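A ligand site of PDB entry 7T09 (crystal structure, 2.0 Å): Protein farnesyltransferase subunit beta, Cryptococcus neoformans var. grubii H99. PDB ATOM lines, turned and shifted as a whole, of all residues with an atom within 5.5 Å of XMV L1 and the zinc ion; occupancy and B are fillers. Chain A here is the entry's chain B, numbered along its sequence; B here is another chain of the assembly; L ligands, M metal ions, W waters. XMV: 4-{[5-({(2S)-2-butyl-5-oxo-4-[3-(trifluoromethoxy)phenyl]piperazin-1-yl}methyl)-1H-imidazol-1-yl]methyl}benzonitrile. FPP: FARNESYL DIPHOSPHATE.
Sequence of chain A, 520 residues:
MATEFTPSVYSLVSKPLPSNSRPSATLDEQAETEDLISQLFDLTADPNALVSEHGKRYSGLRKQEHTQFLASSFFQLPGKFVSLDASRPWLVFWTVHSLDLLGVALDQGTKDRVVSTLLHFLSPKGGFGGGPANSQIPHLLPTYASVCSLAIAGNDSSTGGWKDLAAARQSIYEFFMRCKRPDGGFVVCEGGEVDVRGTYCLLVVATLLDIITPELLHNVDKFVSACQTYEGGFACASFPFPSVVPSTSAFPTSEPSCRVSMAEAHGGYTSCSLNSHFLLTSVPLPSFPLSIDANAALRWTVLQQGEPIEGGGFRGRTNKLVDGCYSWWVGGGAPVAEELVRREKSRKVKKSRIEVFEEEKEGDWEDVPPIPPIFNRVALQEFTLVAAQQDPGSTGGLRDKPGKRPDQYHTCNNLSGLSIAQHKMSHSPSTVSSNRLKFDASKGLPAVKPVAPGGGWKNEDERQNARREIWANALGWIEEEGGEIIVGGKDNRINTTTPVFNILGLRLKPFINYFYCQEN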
ATOM      1  N   LEU A  84      11.293   2.703  33.172  1.00  0.00           N
ATOM      2  CA  LEU A  84      11.715   3.195  31.857  1.00  0.00           C
ATOM      3  C   LEU A  84      12.932   4.111  31.962  1.00  0.00           C
ATOM      4  O   LEU A  84      13.240   4.849  31.012  1.00  0.00           O
ATOM      5  CB  LEU A  84      10.570   3.924  31.170  1.00  0.00           C
ATOM      6  CG  LEU A  84       9.385   3.043  30.747  1.00  0.00           C
ATOM      7  CD1 LEU A  84       8.129   3.874  30.456  1.00  0.00           C
ATOM      8  CD2 LEU A  84       9.778   2.219  29.539  1.00  0.00           C
ATOM      9  N   SER A  87      15.224   4.096  29.181  1.00  0.00           N
ATOM     10  CA  SER A  87      14.572   4.363  27.893  1.00  0.00           C
ATOM     11  C   SER A  87      14.090   5.803  27.819  1.00  0.00           C
ATOM     12  O   SER A  87      13.118   6.099  27.123  1.00  0.00           O
ATOM     13  CB  SER A  87      13.410   3.392  27.663  1.00  0.00           C
ATOM     14  OG  SER A  87      13.865   2.069  27.410  1.00  0.00           O
ATOM     15  N   TRP A  90      13.146   7.346  24.546  1.00  0.00           N
ATOM     16  CA  TRP A  90      11.858   6.910  24.022  1.00  0.00           C
ATOM     17  C   TRP A  90      10.737   7.757  24.601  1.00  0.00           C
ATOM     18  O   TRP A  90       9.777   8.103  23.889  1.00  0.00           O
ATOM     19  CB  TRP A  90      11.612   5.426  24.334  1.00  0.00           C
ATOM     20  CG  TRP A  90      12.459   4.497  23.506  1.00  0.00           C
ATOM     21  CD1 TRP A  90      13.562   3.804  23.910  1.00  0.00           C
ATOM     22  CD2 TRP A  90      12.279   4.180  22.107  1.00  0.00           C
ATOM     23  NE1 TRP A  90      14.070   3.058  22.851  1.00  0.00           N
ATOM     24  CE2 TRP A  90      13.301   3.286  21.746  1.00  0.00           C
ATOM     25  CE3 TRP A  90      11.339   4.573  21.133  1.00  0.00           C
ATOM     26  CZ2 TRP A  90      13.425   2.764  20.447  1.00  0.00           C
ATOM     27  CZ3 TRP A  90      11.457   4.051  19.856  1.00  0.00           C
ATOM     28  CH2 TRP A  90      12.495   3.168  19.521  1.00  0.00           C
ATOM     29  N   TRP A  94       8.326   9.482  22.013  1.00  0.00           N
ATOM     30  CA  TRP A  94       6.869   9.274  22.050  1.00  0.00           C
ATOM     31  C   TRP A  94       6.151  10.600  22.232  1.00  0.00           C
ATOM     32  O   TRP A  94       5.103  10.821  21.613  1.00  0.00           O
ATOM     33  CB  TRP A  94       6.487   8.291  23.162  1.00  0.00           C
ATOM     34  CG  TRP A  94       7.017   6.853  22.957  1.00  0.00           C
ATOM     35  CD1 TRP A  94       7.197   6.194  21.777  1.00  0.00           C
ATOM     36  CD2 TRP A  94       7.426   5.943  23.993  1.00  0.00           C
ATOM     37  NE1 TRP A  94       7.699   4.930  22.007  1.00  0.00           N
ATOM     38  CE2 TRP A  94       7.847   4.749  23.362  1.00  0.00           C
ATOM     39  CE3 TRP A  94       7.476   6.023  25.393  1.00  0.00           C
ATOM     40  CZ2 TRP A  94       8.316   3.640  24.080  1.00  0.00           C
ATOM     41  CZ3 TRP A  94       7.945   4.914  26.111  1.00  0.00           C
ATOM     42  CH2 TRP A  94       8.351   3.742  25.449  1.00  0.00           C
ATOM     43  N   LEU A 141      18.919   1.297  20.440  1.00  0.00           N
ATOM     44  CA  LEU A 141      17.522   1.712  20.396  1.00  0.00           C
ATOM     45  C   LEU A 141      17.364   3.162  20.889  1.00  0.00           C
ATOM     46  O   LEU A 141      16.679   3.949  20.215  1.00  0.00           O
ATOM     47  CB  LEU A 141      16.626   0.753  21.191  1.00  0.00           C
ATOM     48  CG  LEU A 141      16.039  -0.437  20.427  1.00  0.00           C
ATOM     49  CD1 LEU A 141      17.115  -1.245  19.701  1.00  0.00           C
ATOM     50  CD2 LEU A 141      15.252  -1.331  21.388  1.00  0.00           C
ATOM     51  N   ARG A 197      15.234  -5.497  15.901  1.00  0.00           N
ATOM     52  CA  ARG A 197      15.101  -4.140  16.450  1.00  0.00           C
ATOM     53  C   ARG A 197      16.419  -3.391  16.336  1.00  0.00           C
ATOM     54  O   ARG A 197      16.443  -2.197  15.984  1.00  0.00           O
ATOM     55  CB  ARG A 197      14.644  -4.157  17.919  1.00  0.00           C
ATOM     56  CG  ARG A 197      13.313  -4.845  18.225  1.00  0.00           C
ATOM     57  CD  ARG A 197      13.136  -5.004  19.743  1.00  0.00           C
ATOM     58  NE  ARG A 197      14.318  -5.637  20.318  1.00  0.00           N
ATOM     59  CZ  ARG A 197      14.816  -5.381  21.526  1.00  0.00           C
ATOM     60  NH1 ARG A 197      14.223  -4.505  22.333  1.00  0.00           N
ATOM     61  NH2 ARG A 197      15.923  -6.005  21.925  1.00  0.00           N
ATOM     62  N   ASP A 323      -4.678  -4.771  19.707  1.00  0.00           N
ATOM     63  CA  ASP A 323      -3.981  -3.819  20.565  1.00  0.00           C
ATOM     64  C   ASP A 323      -3.658  -2.599  19.707  1.00  0.00           C
ATOM     65  O   ASP A 323      -3.076  -2.732  18.626  1.00  0.00           O
ATOM     66  CB  ASP A 323      -2.697  -4.478  21.142  1.00  0.00           C
ATOM     67  CG  ASP A 323      -1.836  -3.521  21.992  1.00  0.00           C
ATOM     68  OD1 ASP A 323      -1.018  -4.031  22.802  1.00  0.00           O
ATOM     69  OD2 ASP A 323      -1.948  -2.280  21.868  1.00  0.00           O
ATOM     70  N   GLY A 324      -4.025  -1.415  20.213  1.00  0.00           N
ATOM     71  CA  GLY A 324      -3.869  -0.205  19.421  1.00  0.00           C
ATOM     72  C   GLY A 324      -2.454   0.075  18.938  1.00  0.00           C
ATOM     73  O   GLY A 324      -2.280   0.673  17.873  1.00  0.00           O
ATOM     74  N   CYS A 325      -1.422  -0.353  19.693  1.00  0.00           N
ATOM     75  CA  CYS A 325      -0.075   0.000  19.254  1.00  0.00           C
ATOM     76  C   CYS A 325       0.301  -0.699  17.940  1.00  0.00           C
ATOM     77  O   CYS A 325       1.123  -0.170  17.188  1.00  0.00           O
ATOM     78  CB  CYS A 325       0.982  -0.285  20.336  1.00  0.00           C
ATOM     79  SG  CYS A 325       1.225  -2.067  20.769  1.00  0.00           S
ATOM     80  N   TYR A 326      -0.314  -1.847  17.639  1.00  0.00           N
ATOM     81  CA  TYR A 326      -0.048  -2.518  16.367  1.00  0.00           C
ATOM     82  C   TYR A 326      -0.674  -1.818  15.177  1.00  0.00           C
ATOM     83  O   TYR A 326      -0.437  -2.239  14.045  1.00  0.00           O
ATOM     84  CB  TYR A 326      -0.521  -3.977  16.451  1.00  0.00           C
ATOM     85  CG  TYR A 326       0.200  -4.706  17.551  1.00  0.00           C
ATOM     86  CD1 TYR A 326       1.595  -4.688  17.623  1.00  0.00           C
ATOM     87  CD2 TYR A 326      -0.496  -5.366  18.558  1.00  0.00           C
ATOM     88  CE1 TYR A 326       2.272  -5.333  18.663  1.00  0.00           C
ATOM     89  CE2 TYR A 326       0.176  -6.014  19.606  1.00  0.00           C
ATOM     90  CZ  TYR A 326       1.558  -5.993  19.657  1.00  0.00           C
ATOM     91  OH  TYR A 326       2.222  -6.647  20.685  1.00  0.00           O
ATOM     92  N   TRP A 329       2.763  -0.755  14.172  1.00  0.00           N
ATOM     93  CA  TRP A 329       3.735  -1.816  13.872  1.00  0.00           C
ATOM     94  C   TRP A 329       3.257  -2.700  12.724  1.00  0.00           C
ATOM     95  O   TRP A 329       4.056  -3.080  11.858  1.00  0.00           O
ATOM     96  CB  TRP A 329       4.025  -2.673  15.111  1.00  0.00           C
ATOM     97  CG  TRP A 329       4.572  -1.878  16.261  1.00  0.00           C
ATOM     98  CD1 TRP A 329       3.989  -1.728  17.483  1.00  0.00           C
ATOM     99  CD2 TRP A 329       5.788  -1.129  16.300  1.00  0.00           C
ATOM    100  NE1 TRP A 329       4.766  -0.923  18.287  1.00  0.00           N
ATOM    101  CE2 TRP A 329       5.873  -0.536  17.575  1.00  0.00           C
ATOM    102  CE3 TRP A 329       6.823  -0.895  15.376  1.00  0.00           C
ATOM    103  CZ2 TRP A 329       6.957   0.267  17.970  1.00  0.00           C
ATOM    104  CZ3 TRP A 329       7.897  -0.075  15.769  1.00  0.00           C
ATOM    105  CH2 TRP A 329       7.954   0.482  17.053  1.00  0.00           C
ATOM    106  N   ASP A 400      -3.850   0.585  24.808  1.00  0.00           N
ATOM    107  CA  ASP A 400      -3.859  -0.751  24.189  1.00  0.00           C
ATOM    108  C   ASP A 400      -5.306  -1.095  23.801  1.00  0.00           C
ATOM    109  O   ASP A 400      -5.567  -1.252  22.671  1.00  0.00           O
ATOM    110  CB  ASP A 400      -3.250  -1.745  25.170  1.00  0.00           C
ATOM    111  CG  ASP A 400      -3.589  -3.202  24.976  1.00  0.00           C
ATOM    112  OD1 ASP A 400      -4.190  -3.515  24.017  1.00  0.00           O
ATOM    113  OD2 ASP A 400      -3.179  -3.960  25.763  1.00  0.00           O
ATOM    114  N   ASP A 407      -0.795   5.307  28.014  1.00  0.00           N
ATOM    115  CA  ASP A 407       0.599   5.631  28.274  1.00  0.00           C
ATOM    116  C   ASP A 407       1.199   6.293  27.037  1.00  0.00           C
ATOM    117  O   ASP A 407       0.591   6.336  25.962  1.00  0.00           O
ATOM    118  CB  ASP A 407       1.386   4.380  28.706  1.00  0.00           C
ATOM    119  CG  ASP A 407       1.380   3.299  27.641  1.00  0.00           C
ATOM    120  OD1 ASP A 407       1.783   3.586  26.499  1.00  0.00           O
ATOM    121  OD2 ASP A 407       0.995   2.137  27.934  1.00  0.00           O
ATOM    122  N   GLN A 408       2.406   6.850  27.210  1.00  0.00           N
ATOM    123  CA  GLN A 408       3.041   7.569  26.112  1.00  0.00           C
ATOM    124  C   GLN A 408       3.330   6.669  24.911  1.00  0.00           C
ATOM    125  O   GLN A 408       3.222   7.110  23.761  1.00  0.00           O
ATOM    126  CB  GLN A 408       4.328   8.250  26.595  1.00  0.00           C
ATOM    127  CG  GLN A 408       4.141   9.334  27.662  1.00  0.00           C
ATOM    128  CD  GLN A 408       4.037   8.769  29.082  1.00  0.00           C
ATOM    129  OE1 GLN A 408       3.826   7.563  29.287  1.00  0.00           O
ATOM    130  NE2 GLN A 408       4.209   9.635  30.074  1.00  0.00           N
ATOM    131  N   TYR A 409       3.686   5.400  25.162  1.00  0.00           N
ATOM    132  CA  TYR A 409       4.008   4.485  24.069  1.00  0.00           C
ATOM    133  C   TYR A 409       2.786   4.156  23.219  1.00  0.00           C
ATOM    134  O   TYR A 409       2.863   4.151  21.990  1.00  0.00           O
ATOM    135  CB  TYR A 409       4.658   3.201  24.634  1.00  0.00           C
ATOM    136  CG  TYR A 409       4.573   1.994  23.720  1.00  0.00           C
ATOM    137  CD1 TYR A 409       5.579   1.735  22.780  1.00  0.00           C
ATOM    138  CD2 TYR A 409       3.507   1.110  23.791  1.00  0.00           C
ATOM    139  CE1 TYR A 409       5.506   0.620  21.921  1.00  0.00           C
ATOM    140  CE2 TYR A 409       3.439  -0.023  22.956  1.00  0.00           C
ATOM    141  CZ  TYR A 409       4.428  -0.244  22.026  1.00  0.00           C
ATOM    142  OH  TYR A 409       4.324  -1.338  21.188  1.00  0.00           O
ATOM    143  N   HIS A 410       1.639   3.887  23.857  1.00  0.00           N
ATOM    144  CA  HIS A 410       0.440   3.646  23.070  1.00  0.00           C
ATOM    145  C   HIS A 410      -0.096   4.935  22.436  1.00  0.00           C
ATOM    146  O   HIS A 410      -0.774   4.880  21.412  1.00  0.00           O
ATOM    147  CB  HIS A 410      -0.635   2.952  23.915  1.00  0.00           C
ATOM    148  CG  HIS A 410      -0.340   1.505  24.180  1.00  0.00           C
ATOM    149  ND1 HIS A 410       0.173   1.053  25.375  1.00  0.00           N
ATOM    150  CD2 HIS A 410      -0.434   0.420  23.376  1.00  0.00           C
ATOM    151  CE1 HIS A 410       0.356  -0.254  25.309  1.00  0.00           C
ATOM    152  NE2 HIS A 410      -0.007  -0.665  24.108  1.00  0.00           N
ATOM    153  N   ASN A 413       2.062   5.290  19.166  1.00  0.00           N
ATOM    154  CA  ASN A 413       1.888   4.272  18.135  1.00  0.00           C
ATOM    155  C   ASN A 413       0.449   4.171  17.663  1.00  0.00           C
ATOM    156  O   ASN A 413       0.219   3.899  16.477  1.00  0.00           O
ATOM    157  CB  ASN A 413       2.419   2.932  18.642  1.00  0.00           C
ATOM    158  CG  ASN A 413       3.945   2.885  18.641  1.00  0.00           C
ATOM    159  OD1 ASN A 413       4.568   2.924  17.592  1.00  0.00           O
ATOM    160  ND2 ASN A 413       4.553   2.832  19.826  1.00  0.00           N
ATOM    161  N   TYR B 123      13.816  -7.934  28.582  1.00  0.00           N
ATOM    162  CA  TYR B 123      14.811  -8.459  27.644  1.00  0.00           C
ATOM    163  C   TYR B 123      16.141  -8.705  28.342  1.00  0.00           C
ATOM    164  O   TYR B 123      16.846  -9.668  28.029  1.00  0.00           O
ATOM    165  CB  TYR B 123      15.051  -7.463  26.500  1.00  0.00           C
ATOM    166  CG  TYR B 123      14.076  -7.416  25.342  1.00  0.00           C
ATOM    167  CD1 TYR B 123      14.244  -8.212  24.207  1.00  0.00           C
ATOM    168  CD2 TYR B 123      13.009  -6.507  25.352  1.00  0.00           C
ATOM    169  CE1 TYR B 123      13.344  -8.129  23.123  1.00  0.00           C
ATOM    170  CE2 TYR B 123      12.118  -6.407  24.279  1.00  0.00           C
ATOM    171  CZ  TYR B 123      12.291  -7.220  23.168  1.00  0.00           C
ATOM    172  OH  TYR B 123      11.408  -7.114  22.114  1.00  0.00           O
HETATM  173  C10 XMV L   1       6.864  -3.464  26.782  1.00  0.00           C
HETATM  174  C13 XMV L   1       3.640  -3.742  25.277  1.00  0.00           C
HETATM  175  C20 XMV L   1       6.207  -3.903  22.740  1.00  0.00           C
HETATM  176  C21 XMV L   1       7.499  -3.498  22.412  1.00  0.00           C
HETATM  177  C22 XMV L   1       8.602  -4.219  22.872  1.00  0.00           C
HETATM  178  C24 XMV L   1       7.127  -5.770  23.975  1.00  0.00           C
HETATM  179  C28 XMV L   1       9.419  -0.378  23.872  1.00  0.00           C
HETATM  180  C01 XMV L   1       4.869   2.698  28.607  1.00  0.00           C
HETATM  181  C02 XMV L   1       5.189   1.203  28.740  1.00  0.00           C
HETATM  182  C03 XMV L   1       5.055   0.464  27.407  1.00  0.00           C
HETATM  183  C04 XMV L   1       5.508  -1.015  27.475  1.00  0.00           C
HETATM  184  C05 XMV L   1       5.562  -1.683  26.006  1.00  0.00           C
HETATM  185  C06 XMV L   1       6.657  -1.039  25.224  1.00  0.00           C
HETATM  186  C08 XMV L   1       8.170  -2.639  26.404  1.00  0.00           C
HETATM  187  C12 XMV L   1       4.660  -3.731  26.442  1.00  0.00           C
HETATM  188  C14 XMV L   1       2.544  -2.906  25.186  1.00  0.00           C
HETATM  189  C16 XMV L   1       2.591  -4.191  23.424  1.00  0.00           C
HETATM  190  C18 XMV L   1       4.618  -5.575  23.896  1.00  0.00           C
HETATM  191  C19 XMV L   1       6.025  -5.049  23.516  1.00  0.00           C
HETATM  192  C23 XMV L   1       8.422  -5.352  23.652  1.00  0.00           C
HETATM  193  C25 XMV L   1      10.028  -3.770  22.524  1.00  0.00           C
HETATM  194  C27 XMV L   1       9.152  -0.595  25.213  1.00  0.00           C
HETATM  195  C29 XMV L   1      10.498   0.393  23.459  1.00  0.00           C
HETATM  196  C30 XMV L   1      11.323   0.937  24.431  1.00  0.00           C
HETATM  197  C31 XMV L   1      11.074   0.720  25.785  1.00  0.00           C
HETATM  198  C32 XMV L   1       9.982  -0.049  26.177  1.00  0.00           C
HETATM  199  C34 XMV L   1       9.713   0.630  21.173  1.00  0.00           C
HETATM  200  F35 XMV L   1       8.698   1.416  21.638  1.00  0.00           F
HETATM  201  F36 XMV L   1       9.233  -0.621  20.942  1.00  0.00           F
HETATM  202  F37 XMV L   1      10.163   1.130  19.991  1.00  0.00           F
HETATM  203  N07 XMV L   1       8.001  -1.406  25.603  1.00  0.00           N
HETATM  204  N11 XMV L   1       5.735  -3.081  26.072  1.00  0.00           N
HETATM  205  N15 XMV L   1       1.917  -3.197  24.053  1.00  0.00           N
HETATM  206  N17 XMV L   1       3.646  -4.514  24.196  1.00  0.00           N
HETATM  207  N26 XMV L   1      11.081  -3.435  22.273  1.00  0.00           N
HETATM  208  O09 XMV L   1       9.256  -2.996  26.754  1.00  0.00           O
HETATM  209  O33 XMV L   1      10.781   0.602  22.089  1.00  0.00           O
HETATM  210  C1  FPP L   2       5.533  -9.542  22.660  1.00  0.00           C
HETATM  211  O1  FPP L   2       5.037  -8.912  23.823  1.00  0.00           O
HETATM  212  C2  FPP L   2       6.326  -8.558  21.762  1.00  0.00           C
HETATM  213  C3  FPP L   2       7.670  -8.529  21.665  1.00  0.00           C
HETATM  214  C4  FPP L   2       8.556  -9.506  22.446  1.00  0.00           C
HETATM  215  C5  FPP L   2       8.379  -7.513  20.741  1.00  0.00           C
HETATM  216  C6  FPP L   2       7.434  -6.456  20.125  1.00  0.00           C
HETATM  217  C7  FPP L   2       8.257  -5.329  19.446  1.00  0.00           C
HETATM  218  C8  FPP L   2       7.692  -4.185  19.055  1.00  0.00           C
HETATM  219  C10 FPP L   2       6.177  -3.951  19.246  1.00  0.00           C
HETATM  220  C9  FPP L   2       8.454  -3.042  18.386  1.00  0.00           C
HETATM  221  C11 FPP L   2       9.979  -3.150  18.345  1.00  0.00           C
HETATM  222  C12 FPP L   2      10.529  -2.007  17.465  1.00  0.00           C
HETATM  223  C13 FPP L   2      11.508  -1.175  17.807  1.00  0.00           C
HETATM  224  C14 FPP L   2      12.251  -1.251  19.156  1.00  0.00           C
HETATM  225  C15 FPP L   2      11.933  -0.101  16.798  1.00  0.00           C
HETATM  226  PA  FPP L   2       3.572  -9.296  24.509  1.00  0.00           P
HETATM  227  O1A FPP L   2       3.528  -8.573  25.824  1.00  0.00           O
HETATM  228  O2A FPP L   2       3.436 -10.800  24.656  1.00  0.00           O
HETATM  229  O3A FPP L   2       2.357  -8.735  23.582  1.00  0.00           O
HETATM  230  PB  FPP L   2       1.448  -9.551  22.497  1.00  0.00           P
HETATM  231  O1B FPP L   2       0.473 -10.382  23.292  1.00  0.00           O
HETATM  232  O2B FPP L   2       2.285 -10.393  21.583  1.00  0.00           O
HETATM  233  O3B FPP L   2       0.723  -8.472  21.692  1.00  0.00           O
HETATM  234 ZN    ZN M   1       0.360  -2.364  22.904  1.00  0.00          ZN
HETATM  235  O   HOH W   1       9.640  -5.739  27.637  1.00  0.00           O
HETATM  236  O   HOH W   2       1.321  -6.611  25.654  1.00  0.00           O
HETATM  237  O   HOH W   3       7.770   3.440  19.564  1.00  0.00           O
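OD1 of Asp 407 sits at hydrogen-bond distance from N of His 410 (2.7 Å). OH of Tyr 409 sits close to SG of Cys 325, at 3.2 Å. The side-chain carboxylate of Asp 407 lies within hydrogen-bond range of the backbone NH of Tyr 409, 2.9 Å away. The side-chain hydroxyl (OH) of Tyr 409 sits at hydrogen-bond distance from the indole nitrogen (NE1) of Trp 329. The side-chain amide nitrogen (ND2) of Asn 413 lies within hydrogen-bond range of the backbone carbonyl oxygen (O) of Tyr 409 (3.0 Å).
N26 of XMV L1 sits at hydrogen-bond distance from NH1 of Arg 197 (3.3 Å). An oxygen (O3B) of FPP L2 lies within hydrogen-bond range of the side-chain hydroxyl (OH) of Tyr 326 (2.6 Å).
N15 of XMV L1 binds the zinc ion (2.1 Å). NE2 of His 410 is bound to the zinc ion, 2.1 Å away. OD1 of Asp 323 binds the zinc ion (2.2 Å). SG of Cys 325 is bound to the zinc ion (2.3 Å). OD2 of Asp 323 is bound to the zinc ion (2.5 Å).
Residues that only touch XMV L1: Trp 90, Tyr 409, Trp 94, Ser 87, Tyr 123 of chain B, Asp 407, Tyr 326, Trp 329 and Leu 84. Hydrophobic or aromatic side chains within 4 Å of XMV L1: Leu 84, Trp 90, Trp 94, Trp 329, Tyr 409, His 410 and Tyr 123 of chain B. Within 4 Å of XMV L1: Leu 84, Ser 87, Trp 90, Trp 94, Arg 197, Asp 323, Cys 325, Tyr 326, Trp 329, Asp 407, Tyr 409, His 410 and Tyr 123 of chain B. The nearest printed residue that does not touch XMV L1 is Asn 413 (4.7 Å).
Water W3 bridges NE1 of Trp 94 and ND2 of Asn 413.
Tyr 409 touches the zinc ion. Of the 18 residues printed, 4 come within 4 Å of the zinc ion. The nearest printed residue that does not touch the zinc ion is Asp 400 (4.3 Å).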
